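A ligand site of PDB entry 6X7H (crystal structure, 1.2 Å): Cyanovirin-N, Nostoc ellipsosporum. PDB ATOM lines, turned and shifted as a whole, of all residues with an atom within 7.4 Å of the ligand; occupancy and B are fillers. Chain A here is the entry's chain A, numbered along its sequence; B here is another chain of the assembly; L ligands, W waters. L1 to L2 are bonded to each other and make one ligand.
Merely in contact with the ligand: Thr 75 (3.3 Å), Val 43 (3.4 Å), Glu 56 of chain A (3.4 Å), Glu 41 (3.5 Å) and Gly 45 (3.9 Å).
Of the 25 residues printed, 14 come within 4 Å of the ligand.
Along chain A the residues within 4 Å of the ligand span positions 41 to 78.
The side-chain hydroxyl (OG1) of Thr 57 lies within hydrogen-bond range of the side-chain amide nitrogen (ND2) of Asn 42.
N of Asn 53 lies within hydrogen-bond range of O of Ile 40.
O of Arg 76 is in hydrogen-bond range of NE2 of Gln 78 (3.2 Å).
The guanidinium group (NH2) of Arg 76 lies within salt-bridge range of the side-chain carboxylate (OD2) of Asp 44, 3.7 Å away.
The backbone NH (N) of Phe 54 lies within hydrogen-bond range of the backbone carbonyl oxygen (O) of Ile 40 (3.3 Å).
N of Phe 54 is in hydrogen-bond range of OD1 of Asn 37 (3.0 Å).
The side-chain hydroxyl (OG1) of Thr 75 lies close to the backbone NH (N) of Ala 77, 3.3 Å away.
SG of Cys 73 forms a disulfide with SG of Cys 58, at 2.0 Å.
O2 of LG2 L2 lies within hydrogen-bond range of N of Asn 42 (2.9 Å).
O of Asn 42 is in hydrogen-bond range of O3 of LIG L1 (2.7 Å).
An oxygen (O3) of LG2 L2 lies within hydrogen-bond range of the backbone carbonyl oxygen (O) of Asn 53, 2.7 Å away.
OG1 of Thr 57 lies within hydrogen-bond range of O3 of LG2 L2 (2.8 Å).
O of Lys 74 sits at hydrogen-bond distance from O4 of LIG L1.
NE2 of Gln 78 sits at hydrogen-bond distance from O6 of LIG L1 (2.9 Å).
O of Ser 52 sits at hydrogen-bond distance from O2 of LG2 L2, 2.9 Å away.
The backbone NH (N) of Asp 44 sits at hydrogen-bond distance from an oxygen (O3) of LIG L1.
The backbone NH of Phe 54 sits at hydrogen-bond distance from an oxygen (O2) of LG2 L2, at 3.2 Å.
N of Arg 76 is in hydrogen-bond range of O4 of LIG L1, at 3.4 Å.
Water W7 bridges an oxygen (O3) of LIG L1 (2.7 Å) and the guanidinium group of Arg 76 (2.8 Å).
Water W5 bridges an oxygen (O1) of LG2 L2 (2.8 Å) and the side-chain amide oxygen of Asn 53 (3.1 Å).
Water W6 lies within hydrogen-bond range of N of Ser 52 (2.9 Å), OE1 of Glu 41 (3.3 Å) and O1 of LG2 L2 (3.4 Å).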
ATOM      1  N   ASN A  37     -31.955  17.762 -26.787  1.00  0.00           N
ATOM      2  CA  ASN A  37     -31.414  19.087 -27.055  1.00  0.00           C
ATOM      3  C   ASN A  37     -32.485  20.170 -26.923  1.00  0.00           C
ATOM      4  O   ASN A  37     -32.150  21.348 -26.780  1.00  0.00           O
ATOM      5  CB  ASN A  37     -30.785  19.080 -28.445  1.00  0.00           C
ATOM      6  CG  ASN A  37     -29.832  20.220 -28.646  1.00  0.00           C
ATOM      7  OD1 ASN A  37     -29.027  20.552 -27.784  1.00  0.00           O
ATOM      8  ND2 ASN A  37     -29.912  20.815 -29.824  1.00  0.00           N
ATOM      9  N   ILE A  40     -32.466  20.556 -22.482  1.00  0.00           N
ATOM     10  CA  ILE A  40     -31.269  20.623 -21.658  1.00  0.00           C
ATOM     11  C   ILE A  40     -30.330  21.661 -22.234  1.00  0.00           C
ATOM     12  O   ILE A  40     -30.085  21.696 -23.450  1.00  0.00           O
ATOM     13  CB  ILE A  40     -30.590  19.237 -21.536  1.00  0.00           C
ATOM     14  CG1 ILE A  40     -31.565  18.286 -20.809  1.00  0.00           C
ATOM     15  CG2 ILE A  40     -29.281  19.312 -20.805  1.00  0.00           C
ATOM     16  CD1 ILE A  40     -31.131  16.859 -20.720  1.00  0.00           C
ATOM     17  N   GLU A  41     -29.794  22.512 -21.342  1.00  0.00           N
ATOM     18  CA  GLU A  41     -28.856  23.569 -21.662  1.00  0.00           C
ATOM     19  C   GLU A  41     -27.497  23.266 -21.038  1.00  0.00           C
ATOM     20  O   GLU A  41     -27.422  22.665 -19.960  1.00  0.00           O
ATOM     21  CB  GLU A  41     -29.359  24.912 -21.113  1.00  0.00           C
ATOM     22  CG  GLU A  41     -28.538  26.108 -21.543  1.00  0.00           C
ATOM     23  CD  GLU A  41     -29.006  27.446 -20.995  1.00  0.00           C
ATOM     24  OE1 GLU A  41     -30.162  27.589 -20.523  1.00  0.00           O
ATOM     25  OE2 GLU A  41     -28.201  28.387 -21.046  1.00  0.00           O
ATOM     26  N   ASN A  42     -26.432  23.694 -21.712  1.00  0.00           N
ATOM     27  CA  ASN A  42     -25.099  23.689 -21.124  1.00  0.00           C
ATOM     28  C   ASN A  42     -24.905  25.067 -20.507  1.00  0.00           C
ATOM     29  O   ASN A  42     -24.776  26.052 -21.248  1.00  0.00           O
ATOM     30  CB  ASN A  42     -24.014  23.451 -22.154  1.00  0.00           C
ATOM     31  CG  ASN A  42     -22.634  23.737 -21.634  1.00  0.00           C
ATOM     32  OD1 ASN A  42     -22.420  23.782 -20.423  1.00  0.00           O
ATOM     33  ND2 ASN A  42     -21.674  23.921 -22.531  1.00  0.00           N
ATOM     34  N   VAL A  43     -24.915  25.143 -19.185  1.00  0.00           N
ATOM     35  CA  VAL A  43     -24.725  26.393 -18.450  1.00  0.00           C
ATOM     36  C   VAL A  43     -23.333  26.355 -17.818  1.00  0.00           C
ATOM     37  O   VAL A  43     -23.120  25.724 -16.776  1.00  0.00           O
ATOM     38  CB  VAL A  43     -25.816  26.626 -17.414  1.00  0.00           C
ATOM     39  CG1 VAL A  43     -25.582  27.949 -16.710  1.00  0.00           C
ATOM     40  CG2 VAL A  43     -27.193  26.599 -18.050  1.00  0.00           C
ATOM     41  N   ASP A  44     -22.378  27.018 -18.453  1.00  0.00           N
ATOM     42  CA  ASP A  44     -21.016  27.126 -17.923  1.00  0.00           C
ATOM     43  C   ASP A  44     -20.413  25.760 -17.595  1.00  0.00           C
ATOM     44  O   ASP A  44     -19.680  25.614 -16.625  1.00  0.00           O
ATOM     45  CB  ASP A  44     -20.963  28.044 -16.699  1.00  0.00           C
ATOM     46  CG  ASP A  44     -19.557  28.501 -16.367  1.00  0.00           C
ATOM     47  OD1 ASP A  44     -18.723  28.667 -17.283  1.00  0.00           O
ATOM     48  OD2 ASP A  44     -19.289  28.702 -15.164  1.00  0.00           O
ATOM     49  N   GLY A  45     -20.667  24.773 -18.456  1.00  0.00           N
ATOM     50  CA  GLY A  45     -20.105  23.454 -18.299  1.00  0.00           C
ATOM     51  C   GLY A  45     -21.019  22.451 -17.629  1.00  0.00           C
ATOM     52  O   GLY A  45     -20.695  21.266 -17.648  1.00  0.00           O
ATOM     53  N   SER A  46     -22.150  22.882 -17.079  1.00  0.00           N
ATOM     54  CA  SER A  46     -23.056  21.998 -16.364  1.00  0.00           C
ATOM     55  C   SER A  46     -24.365  21.848 -17.133  1.00  0.00           C
ATOM     56  O   SER A  46     -24.947  22.850 -17.567  1.00  0.00           O
ATOM     57  CB  SER A  46     -23.351  22.586 -14.986  1.00  0.00           C
ATOM     58  OG  SER A  46     -22.224  22.539 -14.125  1.00  0.00           O
ATOM     59  N   LEU A  47     -24.824  20.610 -17.292  1.00  0.00           N
ATOM     60  CA  LEU A  47     -26.114  20.362 -17.903  1.00  0.00           C
ATOM     61  C   LEU A  47     -27.247  20.749 -16.961  1.00  0.00           C
ATOM     62  O   LEU A  47     -27.258  20.336 -15.794  1.00  0.00           O
ATOM     63  CB  LEU A  47     -26.241  18.885 -18.259  1.00  0.00           C
ATOM     64  CG  LEU A  47     -25.251  18.391 -19.315  1.00  0.00           C
ATOM     65  CD1 LEU A  47     -25.209  16.861 -19.360  1.00  0.00           C
ATOM     66  CD2 LEU A  47     -25.569  19.006 -20.674  1.00  0.00           C
ATOM     67  N   GLY A  51     -33.554  25.079 -20.406  1.00  0.00           N
ATOM     68  CA  GLY A  51     -32.961  25.689 -21.567  1.00  0.00           C
ATOM     69  C   GLY A  51     -32.800  24.650 -22.626  1.00  0.00           C
ATOM     70  O   GLY A  51     -33.375  23.563 -22.553  1.00  0.00           O
ATOM     71  N   SER A  52     -31.990  24.968 -23.623  1.00  0.00           N
ATOM     72  CA  SER A  52     -31.848  24.086 -24.769  1.00  0.00           C
ATOM     73  C   SER A  52     -30.440  24.198 -25.337  1.00  0.00           C
ATOM     74  O   SER A  52     -29.632  25.011 -24.899  1.00  0.00           O
ATOM     75  CB  SER A  52     -32.837  24.442 -25.893  1.00  0.00           C
ATOM     76  OG  SER A  52     -34.166  24.635 -25.416  1.00  0.00           O
ATOM     77  N   ASN A  53     -30.182  23.381 -26.364  1.00  0.00           N
ATOM     78  CA  ASN A  53     -29.042  23.552 -27.263  1.00  0.00           C
ATOM     79  C   ASN A  53     -27.714  23.078 -26.697  1.00  0.00           C
ATOM     80  O   ASN A  53     -26.664  23.410 -27.272  1.00  0.00           O
ATOM     81  CB  ASN A  53     -28.949  24.991 -27.785  1.00  0.00           C
ATOM     82  CG  ASN A  53     -30.222  25.432 -28.477  1.00  0.00           C
ATOM     83  OD1 ASN A  53     -30.772  26.514 -28.188  1.00  0.00           O
ATOM     84  ND2 ASN A  53     -30.700  24.621 -29.364  1.00  0.00           N
ATOM     85  N   PHE A  54     -27.716  22.236 -25.665  1.00  0.00           N
ATOM     86  CA  PHE A  54     -26.470  21.768 -25.076  1.00  0.00           C
ATOM     87  C   PHE A  54     -25.569  21.065 -26.088  1.00  0.00           C
ATOM     88  O   PHE A  54     -24.345  21.110 -25.940  1.00  0.00           O
ATOM     89  CB  PHE A  54     -26.733  20.848 -23.876  1.00  0.00           C
ATOM     90  CG  PHE A  54     -27.084  19.417 -24.231  1.00  0.00           C
ATOM     91  CD1 PHE A  54     -28.407  19.052 -24.498  1.00  0.00           C
ATOM     92  CD2 PHE A  54     -26.108  18.437 -24.250  1.00  0.00           C
ATOM     93  CE1 PHE A  54     -28.717  17.729 -24.785  1.00  0.00           C
ATOM     94  CE2 PHE A  54     -26.423  17.108 -24.560  1.00  0.00           C
ATOM     95  CZ  PHE A  54     -27.722  16.771 -24.818  1.00  0.00           C
ATOM     96  N   ILE A  55     -26.137  20.434 -27.123  1.00  0.00           N
ATOM     97  CA  ILE A  55     -25.316  19.591 -28.003  1.00  0.00           C
ATOM     98  C   ILE A  55     -24.326  20.435 -28.810  1.00  0.00           C
ATOM     99  O   ILE A  55     -23.344  19.886 -29.319  1.00  0.00           O
ATOM    100  CB  ILE A  55     -26.239  18.668 -28.849  1.00  0.00           C
ATOM    101  CG1 ILE A  55     -25.520  17.383 -29.287  1.00  0.00           C
ATOM    102  CG2 ILE A  55     -26.779  19.451 -30.041  1.00  0.00           C
ATOM    103  CD1 ILE A  55     -25.086  16.488 -28.163  1.00  0.00           C
ATOM    104  N   GLU A  56     -24.545  21.747 -28.911  1.00  0.00           N
ATOM    105  CA  GLU A  56     -23.617  22.594 -29.664  1.00  0.00           C
ATOM    106  C   GLU A  56     -22.279  22.783 -28.962  1.00  0.00           C
ATOM    107  O   GLU A  56     -21.297  23.144 -29.621  1.00  0.00           O
ATOM    108  CB  GLU A  56     -24.228  23.973 -29.882  1.00  0.00           C
ATOM    109  CG  GLU A  56     -25.459  23.982 -30.727  1.00  0.00           C
ATOM    110  CD  GLU A  56     -26.069  25.361 -30.869  1.00  0.00           C
ATOM    111  OE1 GLU A  56     -25.335  26.369 -30.722  1.00  0.00           O
ATOM    112  OE2 GLU A  56     -27.277  25.436 -31.144  1.00  0.00           O
ATOM    113  N   THR A  57     -22.214  22.564 -27.649  1.00  0.00           N
ATOM    114  CA  THR A  57     -21.020  22.860 -26.860  1.00  0.00           C
ATOM    115  C   THR A  57     -20.667  21.733 -25.915  1.00  0.00           C
ATOM    116  O   THR A  57     -19.915  21.934 -24.966  1.00  0.00           O
ATOM    117  CB  THR A  57     -21.172  24.184 -26.104  1.00  0.00           C
ATOM    118  OG1 THR A  57     -22.332  24.113 -25.256  1.00  0.00           O
ATOM    119  CG2 THR A  57     -21.289  25.348 -27.057  1.00  0.00           C
ATOM    120  N   CYS A  58     -21.190  20.540 -26.176  1.00  0.00           N
ATOM    121  CA  CYS A  58     -20.871  19.357 -25.407  1.00  0.00           C
ATOM    122  C   CYS A  58     -20.500  18.232 -26.357  1.00  0.00           C
ATOM    123  O   CYS A  58     -20.854  18.250 -27.539  1.00  0.00           O
ATOM    124  CB  CYS A  58     -22.060  18.928 -24.554  1.00  0.00           C
ATOM    125  SG  CYS A  58     -22.666  20.156 -23.358  1.00  0.00           S
ATOM    126  N   CYS A  73     -18.752  19.087 -21.363  1.00  0.00           N
ATOM    127  CA  CYS A  73     -19.280  20.343 -21.870  1.00  0.00           C
ATOM    128  C   CYS A  73     -18.307  21.475 -21.633  1.00  0.00           C
ATOM    129  O   CYS A  73     -17.593  21.494 -20.636  1.00  0.00           O
ATOM    130  CB  CYS A  73     -20.605  20.706 -21.176  1.00  0.00           C
ATOM    131  SG  CYS A  73     -21.977  19.604 -21.533  1.00  0.00           S
ATOM    132  N   LYS A  74     -18.336  22.451 -22.522  1.00  0.00           N
ATOM    133  CA  LYS A  74     -17.469  23.610 -22.421  1.00  0.00           C
ATOM    134  C   LYS A  74     -18.006  24.642 -21.441  1.00  0.00           C
ATOM    135  O   LYS A  74     -19.187  25.006 -21.485  1.00  0.00           O
ATOM    136  CB  LYS A  74     -17.328  24.281 -23.788  1.00  0.00           C
ATOM    137  CG  LYS A  74     -16.482  23.511 -24.789  1.00  0.00           C
ATOM    138  CD  LYS A  74     -16.030  24.398 -25.953  1.00  0.00           C
ATOM    139  CE  LYS A  74     -17.209  25.054 -26.665  1.00  0.00           C
ATOM    140  NZ  LYS A  74     -16.750  25.863 -27.833  1.00  0.00           N
ATOM    141  N   THR A  75     -17.128  25.152 -20.598  1.00  0.00           N
ATOM    142  CA  THR A  75     -17.421  26.296 -19.762  1.00  0.00           C
ATOM    143  C   THR A  75     -17.420  27.573 -20.620  1.00  0.00           C
ATOM    144  O   THR A  75     -17.021  27.569 -21.787  1.00  0.00           O
ATOM    145  CB  THR A  75     -16.365  26.439 -18.660  1.00  0.00           C
ATOM    146  OG1 THR A  75     -15.116  26.746 -19.289  1.00  0.00           O
ATOM    147  CG2 THR A  75     -16.262  25.167 -17.858  1.00  0.00           C
ATOM    148  N   ARG A  76     -17.825  28.688 -20.025  1.00  0.00           N
ATOM    149  CA  ARG A  76     -17.788  29.945 -20.773  1.00  0.00           C
ATOM    150  C   ARG A  76     -16.356  30.281 -21.204  1.00  0.00           C
ATOM    151  O   ARG A  76     -16.155  30.879 -22.265  1.00  0.00           O
ATOM    152  CB  ARG A  76     -18.396  31.081 -19.964  1.00  0.00           C
ATOM    153  CG  ARG A  76     -19.909  31.032 -19.932  1.00  0.00           C
ATOM    154  CD  ARG A  76     -20.527  32.237 -19.279  1.00  0.00           C
ATOM    155  NE  ARG A  76     -20.351  32.274 -17.820  1.00  0.00           N
ATOM    156  CZ  ARG A  76     -21.245  31.841 -16.937  1.00  0.00           C
ATOM    157  NH1 ARG A  76     -22.377  31.293 -17.350  1.00  0.00           N
ATOM    158  NH2 ARG A  76     -20.994  31.939 -15.640  1.00  0.00           N
ATOM    159  N   ALA A  77     -15.365  29.879 -20.399  1.00  0.00           N
ATOM    160  CA  ALA A  77     -13.943  30.083 -20.706  1.00  0.00           C
ATOM    161  C   ALA A  77     -13.387  29.025 -21.627  1.00  0.00           C
ATOM    162  O   ALA A  77     -12.167  28.971 -21.843  1.00  0.00           O
ATOM    163  CB  ALA A  77     -13.142  30.145 -19.402  1.00  0.00           C
ATOM    164  N   GLN A  78     -14.253  28.169 -22.176  1.00  0.00           N
ATOM    165  CA  GLN A  78     -13.914  27.281 -23.273  1.00  0.00           C
ATOM    166  C   GLN A  78     -13.103  26.075 -22.828  1.00  0.00           C
ATOM    167  O   GLN A  78     -12.348  25.523 -23.618  1.00  0.00           O
ATOM    168  CB  GLN A  78     -13.216  28.036 -24.404  1.00  0.00           C
ATOM    169  CG  GLN A  78     -14.067  29.183 -24.912  1.00  0.00           C
ATOM    170  CD  GLN A  78     -15.369  28.698 -25.492  1.00  0.00           C
ATOM    171  OE1 GLN A  78     -15.395  28.074 -26.556  1.00  0.00           O
ATOM    172  NE2 GLN A  78     -16.447  28.952 -24.793  1.00  0.00           N
ATOM    173  N   GLN A  79     -13.277  25.642 -21.578  1.00  0.00           N
ATOM    174  CA  GLN A  79     -12.629  24.440 -21.077  1.00  0.00           C
ATOM    175  C   GLN A  79     -13.672  23.343 -20.895  1.00  0.00           C
ATOM    176  O   GLN A  79     -14.789  23.610 -20.435  1.00  0.00           O
ATOM    177  CB  GLN A  79     -11.927  24.721 -19.750  1.00  0.00           C
ATOM    178  CG  GLN A  79     -10.820  25.758 -19.874  1.00  0.00           C
ATOM    179  CD  GLN A  79      -9.981  25.903 -18.629  1.00  0.00           C
ATOM    180  OE1 GLN A  79     -10.275  25.292 -17.598  1.00  0.00           O
ATOM    181  NE2 GLN A  79      -8.921  26.698 -18.709  1.00  0.00           N
ATOM    182  N   GLU B  56     -21.861  22.728 -37.151  1.00  0.00           N
ATOM    183  CA  GLU B  56     -20.861  23.709 -36.757  1.00  0.00           C
ATOM    184  C   GLU B  56     -19.752  23.807 -37.782  1.00  0.00           C
ATOM    185  O   GLU B  56     -19.127  24.873 -37.932  1.00  0.00           O
ATOM    186  CB  GLU B  56     -20.276  23.267 -35.415  1.00  0.00           C
ATOM    187  CG  GLU B  56     -19.387  24.250 -34.663  1.00  0.00           C
ATOM    188  CD  GLU B  56     -19.550  24.058 -33.154  1.00  0.00           C
ATOM    189  OE1 GLU B  56     -18.710  23.365 -32.556  1.00  0.00           O
ATOM    190  OE2 GLU B  56     -20.533  24.575 -32.577  1.00  0.00           O
HETATM  191  C1  LIG L   1     -22.376  29.633 -24.331  1.00  0.00           C
HETATM  192  C2  LIG L   1     -23.284  29.275 -23.178  1.00  0.00           C
HETATM  193  C3  LIG L   1     -22.524  28.773 -21.982  1.00  0.00           C
HETATM  194  C4  LIG L   1     -21.509  27.702 -22.398  1.00  0.00           C
HETATM  195  C5  LIG L   1     -20.638  28.187 -23.584  1.00  0.00           C
HETATM  196  C6  LIG L   1     -19.699  27.133 -24.131  1.00  0.00           C
HETATM  197  O1  LIG L   1     -21.764  30.819 -23.875  1.00  0.00           O
HETATM  198  O2  LIG L   1     -24.120  28.217 -23.588  1.00  0.00           O
HETATM  199  O3  LIG L   1     -23.384  28.289 -20.922  1.00  0.00           O
HETATM  200  O4  LIG L   1     -20.674  27.401 -21.280  1.00  0.00           O
HETATM  201  O5  LIG L   1     -21.474  28.611 -24.660  1.00  0.00           O
HETATM  202  O6  LIG L   1     -19.000  27.651 -25.233  1.00  0.00           O
HETATM  203  C1  LG2 L   2     -25.271  28.434 -24.226  1.00  0.00           C
HETATM  204  C2  LG2 L   2     -26.272  27.348 -23.939  1.00  0.00           C
HETATM  205  C3  LG2 L   2     -25.768  26.045 -24.519  1.00  0.00           C
HETATM  206  C4  LG2 L   2     -25.409  26.176 -25.990  1.00  0.00           C
HETATM  207  C5  LG2 L   2     -24.484  27.404 -26.213  1.00  0.00           C
HETATM  208  C6  LG2 L   2     -24.260  27.627 -27.707  1.00  0.00           C
HETATM  209  O1  LG2 L   2     -27.560  27.660 -24.570  1.00  0.00           O
HETATM  210  O2  LG2 L   2     -26.751  25.029 -24.317  1.00  0.00           O
HETATM  211  O3  LG2 L   2     -24.692  25.030 -26.389  1.00  0.00           O
HETATM  212  O4  LG2 L   2     -25.072  28.575 -25.635  1.00  0.00           O
HETATM  213  O5  LG2 L   2     -23.276  28.618 -27.941  1.00  0.00           O
HETATM  214  O   HOH W   1     -22.033  27.905 -30.009  1.00  0.00           O
HETATM  215  O   HOH W   2     -20.346  28.834 -27.461  1.00  0.00           O
HETATM  216  O   HOH W   3     -24.048  31.203 -27.497  1.00  0.00           O
HETATM  217  O   HOH W   4     -20.919  33.800 -22.680  1.00  0.00           O
HETATM  218  O   HOH W   5     -28.402  28.316 -27.170  1.00  0.00           O
HETATM  219  O   HOH W   6     -30.897  27.657 -23.724  1.00  0.00           O
HETATM  220  O   HOH W   7     -23.959  30.544 -19.492  1.00  0.00           O
